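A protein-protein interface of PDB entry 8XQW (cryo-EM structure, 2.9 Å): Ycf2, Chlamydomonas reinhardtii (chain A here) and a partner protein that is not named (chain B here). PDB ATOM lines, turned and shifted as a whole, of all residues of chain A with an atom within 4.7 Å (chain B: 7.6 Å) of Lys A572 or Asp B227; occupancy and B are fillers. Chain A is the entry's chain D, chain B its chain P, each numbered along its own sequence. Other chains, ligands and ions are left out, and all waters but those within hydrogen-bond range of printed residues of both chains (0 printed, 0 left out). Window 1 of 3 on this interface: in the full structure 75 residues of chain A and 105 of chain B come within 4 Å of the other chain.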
ATOM      1  N   ILE A 544     -27.814  -7.418 -32.899  1.00  0.00           N
ATOM      2  CA  ILE A 544     -29.268  -7.464 -32.990  1.00  0.00           C
ATOM      3  C   ILE A 544     -29.857  -6.974 -31.674  1.00  0.00           C
ATOM      4  O   ILE A 544     -29.141  -6.551 -30.765  1.00  0.00           O
ATOM      5  CB  ILE A 544     -29.810  -8.871 -33.323  1.00  0.00           C
ATOM      6  CG1 ILE A 544     -29.557  -9.834 -32.172  1.00  0.00           C
ATOM      7  CG2 ILE A 544     -29.223  -9.407 -34.607  1.00  0.00           C
ATOM      8  CD1 ILE A 544     -30.346 -11.108 -32.285  1.00  0.00           C
ATOM      9  N   SER A 545     -31.182  -7.005 -31.595  1.00  0.00           N
ATOM     10  CA  SER A 545     -31.907  -6.740 -30.361  1.00  0.00           C
ATOM     11  C   SER A 545     -33.309  -7.332 -30.445  1.00  0.00           C
ATOM     12  O   SER A 545     -34.225  -6.684 -30.962  1.00  0.00           O
ATOM     13  CB  SER A 545     -31.979  -5.244 -30.084  1.00  0.00           C
ATOM     14  OG  SER A 545     -30.764  -4.793 -29.520  1.00  0.00           O
ATOM     15  N   SER A 549     -32.974  -3.884 -23.919  1.00  0.00           N
ATOM     16  CA  SER A 549     -31.868  -4.356 -23.097  1.00  0.00           C
ATOM     17  C   SER A 549     -32.217  -4.336 -21.616  1.00  0.00           C
ATOM     18  O   SER A 549     -31.899  -5.283 -20.889  1.00  0.00           O
ATOM     19  CB  SER A 549     -30.621  -3.515 -23.349  1.00  0.00           C
ATOM     20  OG  SER A 549     -30.457  -2.557 -22.320  1.00  0.00           O
ATOM     21  N   ILE A 553     -32.046  -7.362 -18.885  1.00  0.00           N
ATOM     22  CA  ILE A 553     -31.096  -7.167 -17.798  1.00  0.00           C
ATOM     23  C   ILE A 553     -31.761  -7.416 -16.454  1.00  0.00           C
ATOM     24  O   ILE A 553     -31.213  -8.122 -15.602  1.00  0.00           O
ATOM     25  CB  ILE A 553     -30.472  -5.765 -17.877  1.00  0.00           C
ATOM     26  CG1 ILE A 553     -29.275  -5.785 -18.823  1.00  0.00           C
ATOM     27  CG2 ILE A 553     -30.060  -5.283 -16.498  1.00  0.00           C
ATOM     28  CD1 ILE A 553     -28.411  -4.555 -18.746  1.00  0.00           C
ATOM     29  N   LEU A 568     -18.810  -3.185 -18.411  1.00  0.00           N
ATOM     30  CA  LEU A 568     -19.895  -2.991 -19.366  1.00  0.00           C
ATOM     31  C   LEU A 568     -21.148  -2.454 -18.682  1.00  0.00           C
ATOM     32  O   LEU A 568     -21.683  -1.411 -19.078  1.00  0.00           O
ATOM     33  CB  LEU A 568     -20.191  -4.302 -20.090  1.00  0.00           C
ATOM     34  CG  LEU A 568     -19.049  -4.861 -20.935  1.00  0.00           C
ATOM     35  CD1 LEU A 568     -19.574  -5.843 -21.967  1.00  0.00           C
ATOM     36  CD2 LEU A 568     -18.280  -3.741 -21.603  1.00  0.00           C
ATOM     37  N   LEU A 569     -21.639  -3.161 -17.662  1.00  0.00           N
ATOM     38  CA  LEU A 569     -22.797  -2.676 -16.920  1.00  0.00           C
ATOM     39  C   LEU A 569     -22.514  -1.333 -16.265  1.00  0.00           C
ATOM     40  O   LEU A 569     -23.423  -0.503 -16.122  1.00  0.00           O
ATOM     41  CB  LEU A 569     -23.210  -3.701 -15.870  1.00  0.00           C
ATOM     42  CG  LEU A 569     -24.396  -4.574 -16.250  1.00  0.00           C
ATOM     43  CD1 LEU A 569     -24.587  -5.671 -15.227  1.00  0.00           C
ATOM     44  CD2 LEU A 569     -25.637  -3.717 -16.342  1.00  0.00           C
ATOM     45  N   GLN A 570     -21.261  -1.098 -15.871  1.00  0.00           N
ATOM     46  CA  GLN A 570     -20.910   0.196 -15.305  1.00  0.00           C
ATOM     47  C   GLN A 570     -21.108   1.311 -16.320  1.00  0.00           C
ATOM     48  O   GLN A 570     -21.705   2.344 -16.005  1.00  0.00           O
ATOM     49  CB  GLN A 570     -19.474   0.185 -14.798  1.00  0.00           C
ATOM     50  CG  GLN A 570     -19.115   1.428 -14.025  1.00  0.00           C
ATOM     51  CD  GLN A 570     -18.467   2.476 -14.898  1.00  0.00           C
ATOM     52  OE1 GLN A 570     -18.343   2.299 -16.110  1.00  0.00           O
ATOM     53  NE2 GLN A 570     -18.060   3.582 -14.290  1.00  0.00           N
ATOM     54  N   HIS A 571     -20.628   1.125 -17.546  1.00  0.00           N
ATOM     55  CA  HIS A 571     -20.831   2.154 -18.557  1.00  0.00           C
ATOM     56  C   HIS A 571     -22.304   2.285 -18.912  1.00  0.00           C
ATOM     57  O   HIS A 571     -22.782   3.383 -19.207  1.00  0.00           O
ATOM     58  CB  HIS A 571     -19.990   1.855 -19.791  1.00  0.00           C
ATOM     59  CG  HIS A 571     -18.553   2.234 -19.630  1.00  0.00           C
ATOM     60  ND1 HIS A 571     -18.120   3.075 -18.628  1.00  0.00           N
ATOM     61  CD2 HIS A 571     -17.449   1.876 -20.326  1.00  0.00           C
ATOM     62  CE1 HIS A 571     -16.812   3.228 -18.720  1.00  0.00           C
ATOM     63  NE2 HIS A 571     -16.379   2.510 -19.740  1.00  0.00           N
ATOM     64  N   LYS A 572     -23.045   1.177 -18.867  1.00  0.00           N
ATOM     65  CA  LYS A 572     -24.471   1.256 -19.162  1.00  0.00           C
ATOM     66  C   LYS A 572     -25.197   2.149 -18.168  1.00  0.00           C
ATOM     67  O   LYS A 572     -25.890   3.093 -18.565  1.00  0.00           O
ATOM     68  CB  LYS A 572     -25.093  -0.135 -19.180  1.00  0.00           C
ATOM     69  CG  LYS A 572     -24.832  -0.900 -20.455  1.00  0.00           C
ATOM     70  CD  LYS A 572     -25.972  -1.840 -20.762  1.00  0.00           C
ATOM     71  CE  LYS A 572     -27.245  -1.065 -21.008  1.00  0.00           C
ATOM     72  NZ  LYS A 572     -28.289  -1.900 -21.653  1.00  0.00           N
ATOM     73  N   LEU A 573     -25.055   1.885 -16.868  1.00  0.00           N
ATOM     74  CA  LEU A 573     -25.785   2.732 -15.928  1.00  0.00           C
ATOM     75  C   LEU A 573     -25.111   4.093 -15.787  1.00  0.00           C
ATOM     76  O   LEU A 573     -25.701   5.029 -15.239  1.00  0.00           O
ATOM     77  CB  LEU A 573     -25.955   2.063 -14.562  1.00  0.00           C
ATOM     78  CG  LEU A 573     -24.951   2.149 -13.411  1.00  0.00           C
ATOM     79  CD1 LEU A 573     -25.445   1.340 -12.220  1.00  0.00           C
ATOM     80  CD2 LEU A 573     -23.599   1.686 -13.805  1.00  0.00           C
ATOM     81  N   ASN A 574     -23.873   4.220 -16.272  1.00  0.00           N
ATOM     82  CA  ASN A 574     -23.240   5.528 -16.367  1.00  0.00           C
ATOM     83  C   ASN A 574     -23.937   6.386 -17.412  1.00  0.00           C
ATOM     84  O   ASN A 574     -24.207   7.570 -17.184  1.00  0.00           O
ATOM     85  CB  ASN A 574     -21.763   5.354 -16.712  1.00  0.00           C
ATOM     86  CG  ASN A 574     -20.982   6.651 -16.651  1.00  0.00           C
ATOM     87  OD1 ASN A 574     -19.780   6.664 -16.908  1.00  0.00           O
ATOM     88  ND2 ASN A 574     -21.648   7.742 -16.285  1.00  0.00           N
ATOM     89  N   LYS A 575     -24.215   5.810 -18.575  1.00  0.00           N
ATOM     90  CA  LYS A 575     -24.941   6.510 -19.620  1.00  0.00           C
ATOM     91  C   LYS A 575     -26.449   6.441 -19.420  1.00  0.00           C
ATOM     92  O   LYS A 575     -27.198   6.969 -20.247  1.00  0.00           O
ATOM     93  CB  LYS A 575     -24.566   5.951 -20.999  1.00  0.00           C
ATOM     94  CG  LYS A 575     -23.065   5.936 -21.365  1.00  0.00           C
ATOM     95  CD  LYS A 575     -22.175   6.979 -20.669  1.00  0.00           C
ATOM     96  CE  LYS A 575     -22.571   8.429 -20.953  1.00  0.00           C
ATOM     97  NZ  LYS A 575     -21.960   9.347 -19.954  1.00  0.00           N
ATOM     98  N   SER A 576     -26.907   5.813 -18.341  1.00  0.00           N
ATOM     99  CA  SER A 576     -28.328   5.788 -18.022  1.00  0.00           C
ATOM    100  C   SER A 576     -28.855   7.193 -17.729  1.00  0.00           C
ATOM    101  O   SER A 576     -29.864   7.595 -18.325  1.00  0.00           O
ATOM    102  CB  SER A 576     -28.592   4.838 -16.849  1.00  0.00           C
ATOM    103  OG  SER A 576     -29.641   5.310 -16.023  1.00  0.00           O
ATOM    104  N   ALA B 221     -25.235   2.255 -33.187  1.00  0.00           N
ATOM    105  CA  ALA B 221     -25.742   0.959 -32.753  1.00  0.00           C
ATOM    106  C   ALA B 221     -25.653   0.802 -31.244  1.00  0.00           C
ATOM    107  O   ALA B 221     -26.389   0.002 -30.658  1.00  0.00           O
ATOM    108  CB  ALA B 221     -24.977  -0.167 -33.444  1.00  0.00           C
ATOM    109  N   GLU B 222     -24.759   1.544 -30.603  1.00  0.00           N
ATOM    110  CA  GLU B 222     -24.671   1.478 -29.154  1.00  0.00           C
ATOM    111  C   GLU B 222     -25.784   2.273 -28.485  1.00  0.00           C
ATOM    112  O   GLU B 222     -26.461   1.750 -27.594  1.00  0.00           O
ATOM    113  CB  GLU B 222     -23.299   1.972 -28.704  1.00  0.00           C
ATOM    114  CG  GLU B 222     -23.145   2.123 -27.216  1.00  0.00           C
ATOM    115  CD  GLU B 222     -22.392   3.376 -26.855  1.00  0.00           C
ATOM    116  OE1 GLU B 222     -22.758   4.025 -25.856  1.00  0.00           O
ATOM    117  OE2 GLU B 222     -21.434   3.717 -27.579  1.00  0.00           O
ATOM    118  N   GLU B 223     -26.006   3.514 -28.909  1.00  0.00           N
ATOM    119  CA  GLU B 223     -27.076   4.327 -28.349  1.00  0.00           C
ATOM    120  C   GLU B 223     -28.459   3.813 -28.713  1.00  0.00           C
ATOM    121  O   GLU B 223     -29.441   4.230 -28.095  1.00  0.00           O
ATOM    122  CB  GLU B 223     -26.942   5.782 -28.807  1.00  0.00           C
ATOM    123  CG  GLU B 223     -25.533   6.353 -28.721  1.00  0.00           C
ATOM    124  CD  GLU B 223     -24.941   6.304 -27.320  1.00  0.00           C
ATOM    125  OE1 GLU B 223     -25.710   6.277 -26.336  1.00  0.00           O
ATOM    126  OE2 GLU B 223     -23.698   6.302 -27.202  1.00  0.00           O
ATOM    127  N   LEU B 224     -28.558   2.929 -29.698  1.00  0.00           N
ATOM    128  CA  LEU B 224     -29.817   2.293 -30.046  1.00  0.00           C
ATOM    129  C   LEU B 224     -30.102   1.066 -29.198  1.00  0.00           C
ATOM    130  O   LEU B 224     -31.089   0.372 -29.460  1.00  0.00           O
ATOM    131  CB  LEU B 224     -29.815   1.906 -31.524  1.00  0.00           C
ATOM    132  CG  LEU B 224     -31.104   2.197 -32.284  1.00  0.00           C
ATOM    133  CD1 LEU B 224     -31.626   3.577 -31.940  1.00  0.00           C
ATOM    134  CD2 LEU B 224     -30.879   2.066 -33.778  1.00  0.00           C
ATOM    135  N   GLU B 225     -29.258   0.781 -28.206  1.00  0.00           N
ATOM    136  CA  GLU B 225     -29.438  -0.352 -27.299  1.00  0.00           C
ATOM    137  C   GLU B 225     -29.353  -1.685 -28.042  1.00  0.00           C
ATOM    138  O   GLU B 225     -30.156  -2.592 -27.830  1.00  0.00           O
ATOM    139  CB  GLU B 225     -30.762  -0.237 -26.534  1.00  0.00           C
ATOM    140  CG  GLU B 225     -30.879   0.930 -25.541  1.00  0.00           C
ATOM    141  CD  GLU B 225     -29.651   1.166 -24.655  1.00  0.00           C
ATOM    142  OE1 GLU B 225     -28.788   0.274 -24.516  1.00  0.00           O
ATOM    143  OE2 GLU B 225     -29.552   2.273 -24.086  1.00  0.00           O
ATOM    144  N   LEU B 226     -28.366  -1.800 -28.928  1.00  0.00           N
ATOM    145  CA  LEU B 226     -28.144  -3.041 -29.666  1.00  0.00           C
ATOM    146  C   LEU B 226     -27.042  -3.854 -28.990  1.00  0.00           C
ATOM    147  O   LEU B 226     -25.915  -3.956 -29.466  1.00  0.00           O
ATOM    148  CB  LEU B 226     -27.805  -2.739 -31.120  1.00  0.00           C
ATOM    149  CG  LEU B 226     -28.867  -1.994 -31.929  1.00  0.00           C
ATOM    150  CD1 LEU B 226     -28.332  -1.672 -33.296  1.00  0.00           C
ATOM    151  CD2 LEU B 226     -30.128  -2.811 -32.054  1.00  0.00           C
ATOM    152  N   ASP B 227     -27.392  -4.424 -27.840  1.00  0.00           N
ATOM    153  CA  ASP B 227     -26.437  -5.181 -27.031  1.00  0.00           C
ATOM    154  C   ASP B 227     -26.591  -6.689 -27.194  1.00  0.00           C
ATOM    155  O   ASP B 227     -26.934  -7.399 -26.257  1.00  0.00           O
ATOM    156  CB  ASP B 227     -26.573  -4.780 -25.570  1.00  0.00           C
ATOM    157  CG  ASP B 227     -25.876  -3.483 -25.267  1.00  0.00           C
ATOM    158  OD1 ASP B 227     -24.779  -3.259 -25.820  1.00  0.00           O
ATOM    159  OD2 ASP B 227     -26.422  -2.688 -24.479  1.00  0.00           O
ATOM    160  N   TRP B 228     -26.339  -7.195 -28.395  1.00  0.00           N
ATOM    161  CA  TRP B 228     -26.272  -8.635 -28.629  1.00  0.00           C
ATOM    162  C   TRP B 228     -25.197  -8.860 -29.681  1.00  0.00           C
ATOM    163  O   TRP B 228     -25.501  -8.928 -30.871  1.00  0.00           O
ATOM    164  CB  TRP B 228     -27.612  -9.183 -29.094  1.00  0.00           C
ATOM    165  CG  TRP B 228     -28.420  -9.835 -28.032  1.00  0.00           C
ATOM    166  CD1 TRP B 228     -28.415 -11.155 -27.694  1.00  0.00           C
ATOM    167  CD2 TRP B 228     -29.377  -9.205 -27.179  1.00  0.00           C
ATOM    168  NE1 TRP B 228     -29.303 -11.383 -26.675  1.00  0.00           N
ATOM    169  CE2 TRP B 228     -29.908 -10.201 -26.343  1.00  0.00           C
ATOM    170  CE3 TRP B 228     -29.835  -7.895 -27.039  1.00  0.00           C
ATOM    171  CZ2 TRP B 228     -30.871  -9.928 -25.382  1.00  0.00           C
ATOM    172  CZ3 TRP B 228     -30.788  -7.626 -26.086  1.00  0.00           C
ATOM    173  CH2 TRP B 228     -31.296  -8.637 -25.268  1.00  0.00           C
ATOM    174  N   GLY B 229     -23.956  -9.007 -29.247  1.00  0.00           N
ATOM    175  CA  GLY B 229     -22.870  -9.249 -30.169  1.00  0.00           C
ATOM    176  C   GLY B 229     -23.007 -10.600 -30.841  1.00  0.00           C
ATOM    177  O   GLY B 229     -23.817 -11.425 -30.446  1.00  0.00           O
ATOM    178  N   TYR B 260     -25.877 -15.221 -30.874  1.00  0.00           N
ATOM    179  CA  TYR B 260     -25.676 -13.922 -30.257  1.00  0.00           C
ATOM    180  C   TYR B 260     -25.894 -14.042 -28.758  1.00  0.00           C
ATOM    181  O   TYR B 260     -26.687 -14.866 -28.299  1.00  0.00           O
ATOM    182  CB  TYR B 260     -26.632 -12.870 -30.827  1.00  0.00           C
ATOM    183  CG  TYR B 260     -26.574 -12.719 -32.325  1.00  0.00           C
ATOM    184  CD1 TYR B 260     -25.676 -11.851 -32.920  1.00  0.00           C
ATOM    185  CD2 TYR B 260     -27.426 -13.438 -33.143  1.00  0.00           C
ATOM    186  CE1 TYR B 260     -25.624 -11.712 -34.282  1.00  0.00           C
ATOM    187  CE2 TYR B 260     -27.376 -13.305 -34.503  1.00  0.00           C
ATOM    188  CZ  TYR B 260     -26.479 -12.443 -35.067  1.00  0.00           C
ATOM    189  OH  TYR B 260     -26.437 -12.315 -36.431  1.00  0.00           O
ATOM    190  N   ALA B 261     -25.195 -13.202 -27.999  1.00  0.00           N
ATOM    191  CA  ALA B 261     -25.277 -13.228 -26.548  1.00  0.00           C
ATOM    192  C   ALA B 261     -25.111 -11.825 -25.987  1.00  0.00           C
ATOM    193  O   ALA B 261     -24.278 -11.050 -26.455  1.00  0.00           O
ATOM    194  CB  ALA B 261     -24.213 -14.144 -25.949  1.00  0.00           C
ATOM    195  N   HIS B 262     -25.893 -11.521 -24.955  1.00  0.00           N
ATOM    196  CA  HIS B 262     -25.882 -10.195 -24.353  1.00  0.00           C
ATOM    197  C   HIS B 262     -24.534  -9.922 -23.705  1.00  0.00           C
ATOM    198  O   HIS B 262     -24.203 -10.517 -22.679  1.00  0.00           O
ATOM    199  CB  HIS B 262     -27.002 -10.089 -23.325  1.00  0.00           C
ATOM    200  CG  HIS B 262     -27.168  -8.722 -22.742  1.00  0.00           C
ATOM    201  ND1 HIS B 262     -28.335  -8.000 -22.860  1.00  0.00           N
ATOM    202  CD2 HIS B 262     -26.320  -7.949 -22.025  1.00  0.00           C
ATOM    203  CE1 HIS B 262     -28.195  -6.839 -22.247  1.00  0.00           C
ATOM    204  NE2 HIS B 262     -26.981  -6.782 -21.735  1.00  0.00           N
ATOM    205  N   GLU B 263     -23.773  -9.001 -24.275  1.00  0.00           N
ATOM    206  CA  GLU B 263     -22.383  -8.819 -23.874  1.00  0.00           C
ATOM    207  C   GLU B 263     -22.212  -8.209 -22.483  1.00  0.00           C
ATOM    208  O   GLU B 263     -21.316  -8.640 -21.749  1.00  0.00           O
ATOM    209  CB  GLU B 263     -21.647  -7.972 -24.915  1.00  0.00           C
ATOM    210  CG  GLU B 263     -21.761  -8.507 -26.329  1.00  0.00           C
ATOM    211  CD  GLU B 263     -20.416  -8.631 -27.018  1.00  0.00           C
ATOM    212  OE1 GLU B 263     -19.385  -8.382 -26.361  1.00  0.00           O
ATOM    213  OE2 GLU B 263     -20.387  -8.982 -28.216  1.00  0.00           O
ATOM    214  N   PRO B 264     -22.996  -7.201 -22.079  1.00  0.00           N
ATOM    215  CA  PRO B 264     -22.888  -6.737 -20.687  1.00  0.00           C
ATOM    216  C   PRO B 264     -23.146  -7.824 -19.657  1.00  0.00           C
ATOM    217  O   PRO B 264     -22.391  -7.943 -18.682  1.00  0.00           O
ATOM    218  CB  PRO B 264     -23.939  -5.627 -20.615  1.00  0.00           C
ATOM    219  CG  PRO B 264     -23.964  -5.080 -21.968  1.00  0.00           C
ATOM    220  CD  PRO B 264     -23.738  -6.231 -22.903  1.00  0.00           C
ATOM    221  N   LEU B 265     -24.200  -8.619 -19.838  1.00  0.00           N
ATOM    222  CA  LEU B 265     -24.453  -9.710 -18.909  1.00  0.00           C
ATOM    223  C   LEU B 265     -23.346 -10.749 -18.955  1.00  0.00           C
ATOM    224  O   LEU B 265     -23.033 -11.362 -17.933  1.00  0.00           O
ATOM    225  CB  LEU B 265     -25.799 -10.360 -19.207  1.00  0.00           C
ATOM    226  CG  LEU B 265     -27.016  -9.579 -18.724  1.00  0.00           C
ATOM    227  CD1 LEU B 265     -28.292 -10.342 -19.020  1.00  0.00           C
ATOM    228  CD2 LEU B 265     -26.884  -9.293 -17.245  1.00  0.00           C
ATOM    229  N   LEU B 299     -27.826 -15.276 -20.091  1.00  0.00           N
ATOM    230  CA  LEU B 299     -27.323 -14.287 -21.029  1.00  0.00           C
ATOM    231  C   LEU B 299     -28.326 -13.944 -22.117  1.00  0.00           C
ATOM    232  O   LEU B 299     -28.012 -13.135 -22.994  1.00  0.00           O
ATOM    233  CB  LEU B 299     -26.032 -14.778 -21.680  1.00  0.00           C
ATOM    234  CG  LEU B 299     -24.781 -14.824 -20.816  1.00  0.00           C
ATOM    235  CD1 LEU B 299     -23.564 -14.682 -21.689  1.00  0.00           C
ATOM    236  CD2 LEU B 299     -24.817 -13.737 -19.773  1.00  0.00           C
ATOM    237  N   GLY B 300     -29.518 -14.530 -22.083  1.00  0.00           N
ATOM    238  CA  GLY B 300     -30.465 -14.314 -23.161  1.00  0.00           C
ATOM    239  C   GLY B 300     -29.942 -14.788 -24.497  1.00  0.00           C
ATOM    240  O   GLY B 300     -30.164 -14.126 -25.518  1.00  0.00           O
ATOM    241  N   TRP B 355     -33.319  -2.246 -11.893  1.00  0.00           N
ATOM    242  CA  TRP B 355     -31.880  -2.437 -11.728  1.00  0.00           C
ATOM    243  C   TRP B 355     -31.066  -1.150 -11.619  1.00  0.00           C
ATOM    244  O   TRP B 355     -30.065  -1.161 -10.879  1.00  0.00           O
ATOM    245  CB  TRP B 355     -31.337  -3.327 -12.855  1.00  0.00           C
ATOM    246  CG  TRP B 355     -31.214  -2.685 -14.188  1.00  0.00           C
ATOM    247  CD1 TRP B 355     -32.081  -2.797 -15.226  1.00  0.00           C
ATOM    248  CD2 TRP B 355     -30.147  -1.848 -14.642  1.00  0.00           C
ATOM    249  NE1 TRP B 355     -31.627  -2.073 -16.299  1.00  0.00           N
ATOM    250  CE2 TRP B 355     -30.442  -1.479 -15.963  1.00  0.00           C
ATOM    251  CE3 TRP B 355     -28.978  -1.366 -14.055  1.00  0.00           C
ATOM    252  CZ2 TRP B 355     -29.609  -0.655 -16.707  1.00  0.00           C
ATOM    253  CZ3 TRP B 355     -28.155  -0.549 -14.793  1.00  0.00           C
ATOM    254  CH2 TRP B 355     -28.473  -0.200 -16.106  1.00  0.00           C
ATOM    255  N   THR B 514     -15.341  -6.130 -25.998  1.00  0.00           N
ATOM    256  CA  THR B 514     -16.508  -6.664 -26.678  1.00  0.00           C
ATOM    257  C   THR B 514     -16.149  -6.985 -28.118  1.00  0.00           C
ATOM    258  O   THR B 514     -15.305  -6.316 -28.720  1.00  0.00           O
ATOM    259  CB  THR B 514     -17.672  -5.678 -26.664  1.00  0.00           C
ATOM    260  OG1 THR B 514     -18.662  -6.106 -27.605  1.00  0.00           O
ATOM    261  CG2 THR B 514     -17.195  -4.296 -27.051  1.00  0.00           C
ATOM    262  N   LYS B 518     -17.292  -1.727 -30.301  1.00  0.00           N
ATOM    263  CA  LYS B 518     -18.090  -0.503 -30.238  1.00  0.00           C
ATOM    264  C   LYS B 518     -17.641   0.421 -29.127  1.00  0.00           C
ATOM    265  O   LYS B 518     -18.460   0.956 -28.381  1.00  0.00           O
ATOM    266  CB  LYS B 518     -19.560  -0.860 -30.053  1.00  0.00           C
ATOM    267  CG  LYS B 518     -20.161  -1.664 -31.170  1.00  0.00           C
ATOM    268  CD  LYS B 518     -21.140  -2.687 -30.640  1.00  0.00           C
ATOM    269  CE  LYS B 518     -21.964  -2.120 -29.506  1.00  0.00           C
ATOM    270  NZ  LYS B 518     -23.084  -3.024 -29.141  1.00  0.00           N
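The side-chain carboxylate (OD2) of Asp B227 lies within salt-bridge range of the side-chain amino group (NZ) of Lys A572, 3.5 Å away. N of Ile A544 lies within hydrogen-bond range of O of Trp B228. The backbone carbonyl oxygen of Glu B225 sits at hydrogen-bond distance from the side-chain hydroxyl of Ser A545 (2.8 Å). The side-chain carboxylate of Glu B225 is in salt-bridge range of the side-chain amino group of Lys A572, at 3.6 Å.
The backbone NH (N) of Leu B226 sits close to the backbone carbonyl oxygen (O) of Ala B221. The indole nitrogen (NE1) of Trp B228 is in hydrogen-bond range of the backbone carbonyl oxygen (O) of Gly B300. The side-chain amino group (NZ) of Lys B518 is in salt-bridge range of the side-chain carboxylate (OD1) of Asp B227. The backbone NH of His B262 sits close to the backbone carbonyl oxygen of Leu B299, at 3.3 Å. The side-chain carboxylate (OE1) of Glu B263 sits at hydrogen-bond distance from the side-chain hydroxyl (OG1) of Thr B514 (2.7 Å). O of Leu B226 sits at hydrogen-bond distance from NZ of Lys B518, 3.0 Å away.
Among the printed residues, pairs that only touch across the chains: Ile A544 with Leu B226 (3.8 Å), Ile A544 with Tyr B260 (3.8 Å), Ser A545 with Leu B226 (3.2 Å), Ser A545 with Asp B227 (3.8 Å), Ser A549 with Glu B225 (3.95 Å), Ile A553 with His B262 (3.7 Å), Ile A553 with Trp B355 (3.4 Å), Leu A568 with Glu B263 (3.3 Å), Leu A568 with Pro B264 (3.7 Å), Lys A572 with Pro B264 (3.998 Å) and Leu A573 with Trp B355 (3.4 Å).
Of the printed residues of chain B, Ser A545 touches Glu B225 (2.8 Å), Leu B226 (3.2 Å) and Asp B227 (3.8 Å). Of the printed residues of chain B, Lys A572 touches Glu B225 (3.6 Å), Asp B227 (3.5 Å) and Pro B264 (3.998 Å). Printed residues of chain B within 4 Å of Leu A573: Trp B355 (3.4 Å). Lys A575 touches none of the printed residues of chain B. Of the printed residues of chain A, Asp B227 touches Ser A545 and Lys A572. The nearest printed residue of chain B that does not touch Lys A572 is Trp B355 (4.5 Å). The nearest printed residue of chain A that does not touch Trp B228 is Ser A545 (4.1 Å).
Of the 13 printed residues of chain A, 7 touch a printed residue of chain B. Hydrophobic or aromatic side chains of chain A that line the printed part of chain B: Ile A544, Ile A553, Leu A568 and Leu A573. Hydrophobic or aromatic side chains of chain B within 4 Å of the printed part of chain A: Leu B226, Trp B228, Tyr B260, His B262, Pro B264 and Trp B355. Among the printed residues, Asp or Glu carboxylates within 4 Å of a Lys or Arg side-chain nitrogen of the other chain: Lys A572 with Glu B225 and Lys A572 with Asp B227.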
